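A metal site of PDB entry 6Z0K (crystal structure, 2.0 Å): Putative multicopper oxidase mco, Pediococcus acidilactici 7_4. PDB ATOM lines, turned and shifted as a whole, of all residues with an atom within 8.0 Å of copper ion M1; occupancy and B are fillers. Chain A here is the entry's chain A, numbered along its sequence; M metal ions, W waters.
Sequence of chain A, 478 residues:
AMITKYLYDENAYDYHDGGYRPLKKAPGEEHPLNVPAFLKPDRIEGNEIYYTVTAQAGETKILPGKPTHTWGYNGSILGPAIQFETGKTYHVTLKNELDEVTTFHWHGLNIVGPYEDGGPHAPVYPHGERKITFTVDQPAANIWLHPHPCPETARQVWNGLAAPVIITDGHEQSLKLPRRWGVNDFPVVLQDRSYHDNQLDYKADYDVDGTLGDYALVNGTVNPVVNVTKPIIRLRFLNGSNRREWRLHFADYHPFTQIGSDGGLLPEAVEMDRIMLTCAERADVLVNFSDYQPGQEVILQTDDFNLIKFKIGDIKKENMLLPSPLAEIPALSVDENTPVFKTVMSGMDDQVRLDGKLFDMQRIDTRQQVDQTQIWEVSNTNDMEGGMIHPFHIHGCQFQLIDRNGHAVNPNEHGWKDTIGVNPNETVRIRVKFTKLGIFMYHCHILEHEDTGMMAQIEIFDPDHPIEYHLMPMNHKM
The backbone NH of His 393 sits at hydrogen-bond distance from the backbone carbonyl oxygen of His 443 (2.8 Å). N of His 395 sits at hydrogen-bond distance from O of Met 441 (2.9 Å). ND1 of His 395 is in hydrogen-bond range of OD2 of Asp 117 (2.9 Å). A ring nitrogen (ND1) of His 148 lies close to the side-chain carboxylate of Glu 450.
Copper ion M1 is bound by NE2 of His 395, NE2 of His 148, NE2 of His 443 and water W1. Copper ion M1 has four donor atoms within binding distance.
CD2 of His 393 touches copper ion M1, 3.9 Å away. Of the 23 residues printed, 4 come within 4 Å of copper ion M1. The nearest printed residue that does not touch copper ion M1 is His 105 (4.3 Å).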
ATOM      1  N   HIS A 105      -6.128  -0.072 -13.635  1.00  0.00           N
ATOM      2  CA  HIS A 105      -5.913   1.394 -13.663  1.00  0.00           C
ATOM      3  C   HIS A 105      -5.355   1.830 -15.023  1.00  0.00           C
ATOM      4  O   HIS A 105      -4.276   1.349 -15.410  1.00  0.00           O
ATOM      5  CB  HIS A 105      -4.980   1.869 -12.556  1.00  0.00           C
ATOM      6  CG  HIS A 105      -4.771   3.346 -12.573  1.00  0.00           C
ATOM      7  ND1 HIS A 105      -5.822   4.246 -12.508  1.00  0.00           N
ATOM      8  CD2 HIS A 105      -3.649   4.092 -12.688  1.00  0.00           C
ATOM      9  CE1 HIS A 105      -5.357   5.468 -12.559  1.00  0.00           C
ATOM     10  NE2 HIS A 105      -4.030   5.402 -12.680  1.00  0.00           N
ATOM     11  N   HIS A 107      -3.506   4.410 -16.351  1.00  0.00           N
ATOM     12  CA  HIS A 107      -2.588   5.500 -15.925  1.00  0.00           C
ATOM     13  C   HIS A 107      -2.496   6.521 -17.064  1.00  0.00           C
ATOM     14  O   HIS A 107      -1.892   6.199 -18.107  1.00  0.00           O
ATOM     15  CB  HIS A 107      -1.217   4.960 -15.516  1.00  0.00           C
ATOM     16  CG  HIS A 107      -0.244   6.018 -15.141  1.00  0.00           C
ATOM     17  ND1 HIS A 107       0.330   6.084 -13.887  1.00  0.00           N
ATOM     18  CD2 HIS A 107       0.244   7.068 -15.829  1.00  0.00           C
ATOM     19  CE1 HIS A 107       1.141   7.113 -13.825  1.00  0.00           C
ATOM     20  NE2 HIS A 107       1.112   7.737 -15.012  1.00  0.00           N
ATOM     21  N   ASP A 117     -12.020   4.493 -13.027  1.00  0.00           N
ATOM     22  CA  ASP A 117     -10.587   4.852 -12.874  1.00  0.00           C
ATOM     23  C   ASP A 117      -9.758   3.594 -12.574  1.00  0.00           C
ATOM     24  O   ASP A 117      -8.582   3.545 -12.981  1.00  0.00           O
ATOM     25  CB  ASP A 117     -10.380   5.901 -11.785  1.00  0.00           C
ATOM     26  CG  ASP A 117      -8.965   6.442 -11.692  1.00  0.00           C
ATOM     27  OD1 ASP A 117      -8.342   6.652 -12.764  1.00  0.00           O
ATOM     28  OD2 ASP A 117      -8.484   6.646 -10.565  1.00  0.00           O
ATOM     29  N   GLY A 118     -10.351   2.635 -11.861  1.00  0.00           N
ATOM     30  CA  GLY A 118      -9.699   1.350 -11.561  1.00  0.00           C
ATOM     31  C   GLY A 118      -8.604   1.507 -10.530  1.00  0.00           C
ATOM     32  O   GLY A 118      -7.541   0.889 -10.694  1.00  0.00           O
ATOM     33  N   GLY A 119      -8.851   2.331  -9.510  1.00  0.00           N
ATOM     34  CA  GLY A 119      -7.978   2.431  -8.325  1.00  0.00           C
ATOM     35  C   GLY A 119      -8.374   1.387  -7.285  1.00  0.00           C
ATOM     36  O   GLY A 119      -9.097   0.441  -7.591  1.00  0.00           O
ATOM     37  N   PRO A 120      -7.911   1.531  -6.020  1.00  0.00           N
ATOM     38  CA  PRO A 120      -8.206   0.565  -4.970  1.00  0.00           C
ATOM     39  C   PRO A 120      -9.687   0.364  -4.606  1.00  0.00           C
ATOM     40  O   PRO A 120      -9.986  -0.626  -3.978  1.00  0.00           O
ATOM     41  CB  PRO A 120      -7.439   1.088  -3.739  1.00  0.00           C
ATOM     42  CG  PRO A 120      -6.987   2.491  -4.090  1.00  0.00           C
ATOM     43  CD  PRO A 120      -6.959   2.573  -5.598  1.00  0.00           C
ATOM     44  N   HIS A 146      -2.149  -0.814 -15.698  1.00  0.00           N
ATOM     45  CA  HIS A 146      -1.527  -1.650 -14.647  1.00  0.00           C
ATOM     46  C   HIS A 146      -2.461  -1.750 -13.445  1.00  0.00           C
ATOM     47  O   HIS A 146      -3.407  -0.978 -13.318  1.00  0.00           O
ATOM     48  CB  HIS A 146      -0.117  -1.140 -14.318  1.00  0.00           C
ATOM     49  CG  HIS A 146      -0.136   0.149 -13.591  1.00  0.00           C
ATOM     50  ND1 HIS A 146      -0.525   0.245 -12.274  1.00  0.00           N
ATOM     51  CD2 HIS A 146       0.172   1.399 -13.982  1.00  0.00           C
ATOM     52  CE1 HIS A 146      -0.446   1.499 -11.879  1.00  0.00           C
ATOM     53  NE2 HIS A 146      -0.030   2.228 -12.917  1.00  0.00           N
ATOM     54  N   PRO A 147      -2.223  -2.733 -12.539  1.00  0.00           N
ATOM     55  CA  PRO A 147      -3.081  -2.942 -11.378  1.00  0.00           C
ATOM     56  C   PRO A 147      -2.891  -1.866 -10.299  1.00  0.00           C
ATOM     57  O   PRO A 147      -1.823  -1.283 -10.246  1.00  0.00           O
ATOM     58  CB  PRO A 147      -2.668  -4.325 -10.851  1.00  0.00           C
ATOM     59  CG  PRO A 147      -1.253  -4.519 -11.356  1.00  0.00           C
ATOM     60  CD  PRO A 147      -1.129  -3.700 -12.618  1.00  0.00           C
ATOM     61  N   HIS A 148      -3.915  -1.640  -9.488  1.00  0.00           N
ATOM     62  CA  HIS A 148      -3.854  -0.641  -8.385  1.00  0.00           C
ATOM     63  C   HIS A 148      -4.505  -1.143  -7.089  1.00  0.00           C
ATOM     64  O   HIS A 148      -5.050  -0.342  -6.342  1.00  0.00           O
ATOM     65  CB  HIS A 148      -4.490   0.664  -8.878  1.00  0.00           C
ATOM     66  CG  HIS A 148      -3.767   1.873  -8.423  1.00  0.00           C
ATOM     67  ND1 HIS A 148      -3.560   2.153  -7.095  1.00  0.00           N
ATOM     68  CD2 HIS A 148      -3.205   2.890  -9.126  1.00  0.00           C
ATOM     69  CE1 HIS A 148      -2.911   3.289  -6.984  1.00  0.00           C
ATOM     70  NE2 HIS A 148      -2.681   3.761  -8.209  1.00  0.00           N
ATOM     71  N   THR A 153       0.026  -3.476  -5.100  1.00  0.00           N
ATOM     72  CA  THR A 153       0.287  -2.910  -6.455  1.00  0.00           C
ATOM     73  C   THR A 153       1.717  -3.256  -6.905  1.00  0.00           C
ATOM     74  O   THR A 153       1.866  -3.735  -8.034  1.00  0.00           O
ATOM     75  CB  THR A 153       0.025  -1.401  -6.473  1.00  0.00           C
ATOM     76  OG1 THR A 153      -1.356  -1.191  -6.192  1.00  0.00           O
ATOM     77  CG2 THR A 153       0.382  -0.776  -7.808  1.00  0.00           C
ATOM     78  N   HIS A 393       2.452  11.640  -8.961  1.00  0.00           N
ATOM     79  CA  HIS A 393       1.415  11.339  -9.984  1.00  0.00           C
ATOM     80  C   HIS A 393       0.018  11.682  -9.468  1.00  0.00           C
ATOM     81  O   HIS A 393      -0.258  11.390  -8.290  1.00  0.00           O
ATOM     82  CB  HIS A 393       1.501   9.867 -10.414  1.00  0.00           C
ATOM     83  CG  HIS A 393       0.344   9.401 -11.225  1.00  0.00           C
ATOM     84  ND1 HIS A 393       0.024   9.954 -12.449  1.00  0.00           N
ATOM     85  CD2 HIS A 393      -0.568   8.439 -11.006  1.00  0.00           C
ATOM     86  CE1 HIS A 393      -1.037   9.355 -12.943  1.00  0.00           C
ATOM     87  NE2 HIS A 393      -1.422   8.425 -12.074  1.00  0.00           N
ATOM     88  N   ILE A 394      -0.808  12.275 -10.328  1.00  0.00           N
ATOM     89  CA  ILE A 394      -2.245  12.560 -10.040  1.00  0.00           C
ATOM     90  C   ILE A 394      -3.108  11.769 -11.021  1.00  0.00           C
ATOM     91  O   ILE A 394      -2.861  11.865 -12.239  1.00  0.00           O
ATOM     92  CB  ILE A 394      -2.586  14.053 -10.130  1.00  0.00           C
ATOM     93  CG1 ILE A 394      -1.595  14.919  -9.353  1.00  0.00           C
ATOM     94  CG2 ILE A 394      -4.013  14.290  -9.665  1.00  0.00           C
ATOM     95  CD1 ILE A 394      -1.749  16.411  -9.611  1.00  0.00           C
ATOM     96  N   HIS A 395      -4.112  11.073 -10.498  1.00  0.00           N
ATOM     97  CA  HIS A 395      -5.119  10.342 -11.313  1.00  0.00           C
ATOM     98  C   HIS A 395      -6.099  11.320 -11.959  1.00  0.00           C
ATOM     99  O   HIS A 395      -6.284  12.433 -11.437  1.00  0.00           O
ATOM    100  CB  HIS A 395      -5.901   9.338 -10.465  1.00  0.00           C
ATOM    101  CG  HIS A 395      -5.120   8.130 -10.075  1.00  0.00           C
ATOM    102  ND1 HIS A 395      -5.741   6.920  -9.818  1.00  0.00           N
ATOM    103  CD2 HIS A 395      -3.800   7.923  -9.886  1.00  0.00           C
ATOM    104  CE1 HIS A 395      -4.837   6.027  -9.498  1.00  0.00           C
ATOM    105  NE2 HIS A 395      -3.633   6.615  -9.533  1.00  0.00           N
ATOM    106  N   PHE A 440     -10.213  10.483  -6.793  1.00  0.00           N
ATOM    107  CA  PHE A 440      -8.963  10.194  -7.513  1.00  0.00           C
ATOM    108  C   PHE A 440      -7.801  10.148  -6.530  1.00  0.00           C
ATOM    109  O   PHE A 440      -7.851  10.841  -5.490  1.00  0.00           O
ATOM    110  CB  PHE A 440      -8.723  11.249  -8.595  1.00  0.00           C
ATOM    111  CG  PHE A 440      -9.803  11.297  -9.639  1.00  0.00           C
ATOM    112  CD1 PHE A 440      -9.847  10.358 -10.652  1.00  0.00           C
ATOM    113  CD2 PHE A 440     -10.790  12.275  -9.591  1.00  0.00           C
ATOM    114  CE1 PHE A 440     -10.855  10.401 -11.617  1.00  0.00           C
ATOM    115  CE2 PHE A 440     -11.789  12.319 -10.559  1.00  0.00           C
ATOM    116  CZ  PHE A 440     -11.819  11.383 -11.568  1.00  0.00           C
ATOM    117  N   MET A 441      -6.799   9.339  -6.844  1.00  0.00           N
ATOM    118  CA  MET A 441      -5.574   9.212  -6.018  1.00  0.00           C
ATOM    119  C   MET A 441      -4.556  10.258  -6.489  1.00  0.00           C
ATOM    120  O   MET A 441      -4.567  10.619  -7.674  1.00  0.00           O
ATOM    121  CB  MET A 441      -4.921   7.841  -6.139  1.00  0.00           C
ATOM    122  CG  MET A 441      -5.852   6.650  -6.035  1.00  0.00           C
ATOM    123  SD  MET A 441      -6.631   6.474  -4.410  1.00  0.00           S
ATOM    124  CE  MET A 441      -8.286   7.014  -4.809  1.00  0.00           C
ATOM    125  N   TYR A 442      -3.721  10.727  -5.560  1.00  0.00           N
ATOM    126  CA  TYR A 442      -2.404  11.321  -5.889  1.00  0.00           C
ATOM    127  C   TYR A 442      -1.370  10.723  -4.944  1.00  0.00           C
ATOM    128  O   TYR A 442      -1.680  10.510  -3.758  1.00  0.00           O
ATOM    129  CB  TYR A 442      -2.437  12.843  -5.848  1.00  0.00           C
ATOM    130  CG  TYR A 442      -2.944  13.470  -4.565  1.00  0.00           C
ATOM    131  CD1 TYR A 442      -4.299  13.566  -4.313  1.00  0.00           C
ATOM    132  CD2 TYR A 442      -2.073  13.998  -3.623  1.00  0.00           C
ATOM    133  CE1 TYR A 442      -4.785  14.152  -3.154  1.00  0.00           C
ATOM    134  CE2 TYR A 442      -2.532  14.580  -2.454  1.00  0.00           C
ATOM    135  CZ  TYR A 442      -3.893  14.662  -2.218  1.00  0.00           C
ATOM    136  OH  TYR A 442      -4.378  15.235  -1.079  1.00  0.00           O
ATOM    137  N   HIS A 443      -0.187  10.426  -5.484  1.00  0.00           N
ATOM    138  CA  HIS A 443       0.815   9.623  -4.745  1.00  0.00           C
ATOM    139  C   HIS A 443       2.170   9.653  -5.437  1.00  0.00           C
ATOM    140  O   HIS A 443       2.266  10.085  -6.600  1.00  0.00           O
ATOM    141  CB  HIS A 443       0.331   8.173  -4.628  1.00  0.00           C
ATOM    142  CG  HIS A 443       0.061   7.506  -5.932  1.00  0.00           C
ATOM    143  ND1 HIS A 443       1.000   6.704  -6.558  1.00  0.00           N
ATOM    144  CD2 HIS A 443      -1.027   7.507  -6.723  1.00  0.00           C
ATOM    145  CE1 HIS A 443       0.495   6.241  -7.677  1.00  0.00           C
ATOM    146  NE2 HIS A 443      -0.749   6.716  -7.811  1.00  0.00           N
ATOM    147  N   CYS A 444       3.152   9.164  -4.699  1.00  0.00           N
ATOM    148  CA  CYS A 444       4.474   8.786  -5.239  1.00  0.00           C
ATOM    149  C   CYS A 444       4.301   7.536  -6.101  1.00  0.00           C
ATOM    150  O   CYS A 444       3.585   6.613  -5.656  1.00  0.00           O
ATOM    151  CB  CYS A 444       5.448   8.455  -4.130  1.00  0.00           C
ATOM    152  SG  CYS A 444       7.084   8.063  -4.780  1.00  0.00           S
ATOM    153  N   HIS A 445       4.955   7.478  -7.257  1.00  0.00           N
ATOM    154  CA  HIS A 445       4.855   6.314  -8.164  1.00  0.00           C
ATOM    155  C   HIS A 445       6.041   5.361  -8.007  1.00  0.00           C
ATOM    156  O   HIS A 445       6.166   4.441  -8.832  1.00  0.00           O
ATOM    157  CB  HIS A 445       4.686   6.745  -9.621  1.00  0.00           C
ATOM    158  CG  HIS A 445       3.838   5.789 -10.387  1.00  0.00           C
ATOM    159  ND1 HIS A 445       4.318   4.555 -10.801  1.00  0.00           N
ATOM    160  CD2 HIS A 445       2.550   5.851 -10.782  1.00  0.00           C
ATOM    161  CE1 HIS A 445       3.355   3.913 -11.444  1.00  0.00           C
ATOM    162  NE2 HIS A 445       2.273   4.685 -11.435  1.00  0.00           N
ATOM    163  N   LEU A 447       6.512   2.302  -6.393  1.00  0.00           N
ATOM    164  CA  LEU A 447       5.333   1.456  -6.044  1.00  0.00           C
ATOM    165  C   LEU A 447       5.395   0.989  -4.583  1.00  0.00           C
ATOM    166  O   LEU A 447       4.313   0.839  -3.990  1.00  0.00           O
ATOM    167  CB  LEU A 447       5.238   0.288  -7.032  1.00  0.00           C
ATOM    168  CG  LEU A 447       4.994   0.677  -8.488  1.00  0.00           C
ATOM    169  CD1 LEU A 447       4.954  -0.557  -9.372  1.00  0.00           C
ATOM    170  CD2 LEU A 447       3.700   1.477  -8.658  1.00  0.00           C
ATOM    171  N   GLU A 450       4.113   3.927  -2.530  1.00  0.00           N
ATOM    172  CA  GLU A 450       2.643   3.924  -2.732  1.00  0.00           C
ATOM    173  C   GLU A 450       2.016   2.887  -1.801  1.00  0.00           C
ATOM    174  O   GLU A 450       1.072   3.246  -1.061  1.00  0.00           O
ATOM    175  CB  GLU A 450       2.356   3.614  -4.208  1.00  0.00           C
ATOM    176  CG  GLU A 450       0.885   3.533  -4.560  1.00  0.00           C
ATOM    177  CD  GLU A 450       0.667   2.886  -5.916  1.00  0.00           C
ATOM    178  OE1 GLU A 450      -0.286   2.082  -6.035  1.00  0.00           O
ATOM    179  OE2 GLU A 450       1.445   3.176  -6.843  1.00  0.00           O
ATOM    180  N   MET A 455       0.253   8.153  -0.334  1.00  0.00           N
ATOM    181  CA  MET A 455      -0.882   8.284  -1.272  1.00  0.00           C
ATOM    182  C   MET A 455      -2.050   8.926  -0.543  1.00  0.00           C
ATOM    183  O   MET A 455      -2.198   8.691   0.675  1.00  0.00           O
ATOM    184  CB  MET A 455      -1.305   6.919  -1.818  1.00  0.00           C
ATOM    185  CG  MET A 455      -2.539   6.959  -2.720  1.00  0.00           C
ATOM    186  SD  MET A 455      -2.646   5.523  -3.816  1.00  0.00           S
ATOM    187  CE  MET A 455      -3.080   4.252  -2.634  1.00  0.00           C
ATOM    188  N   ALA A 456      -2.830   9.726  -1.261  1.00  0.00           N
ATOM    189  CA  ALA A 456      -3.982  10.471  -0.713  1.00  0.00           C
ATOM    190  C   ALA A 456      -5.110  10.477  -1.724  1.00  0.00           C
ATOM    191  O   ALA A 456      -4.884  10.086  -2.889  1.00  0.00           O
ATOM    192  CB  ALA A 456      -3.555  11.874  -0.360  1.00  0.00           C
HETATM  193 CU    CU M   1      -2.148   5.588  -8.841  1.00  0.00          CU
HETATM  194 CU    CU M   2      -2.517   6.774 -12.389  1.00  0.00          CU
HETATM  195 CU    CU M   3       0.433   4.378 -12.667  1.00  0.00          CU
HETATM  196  O   HOH W   1      -1.030   4.913 -10.797  1.00  0.00           O
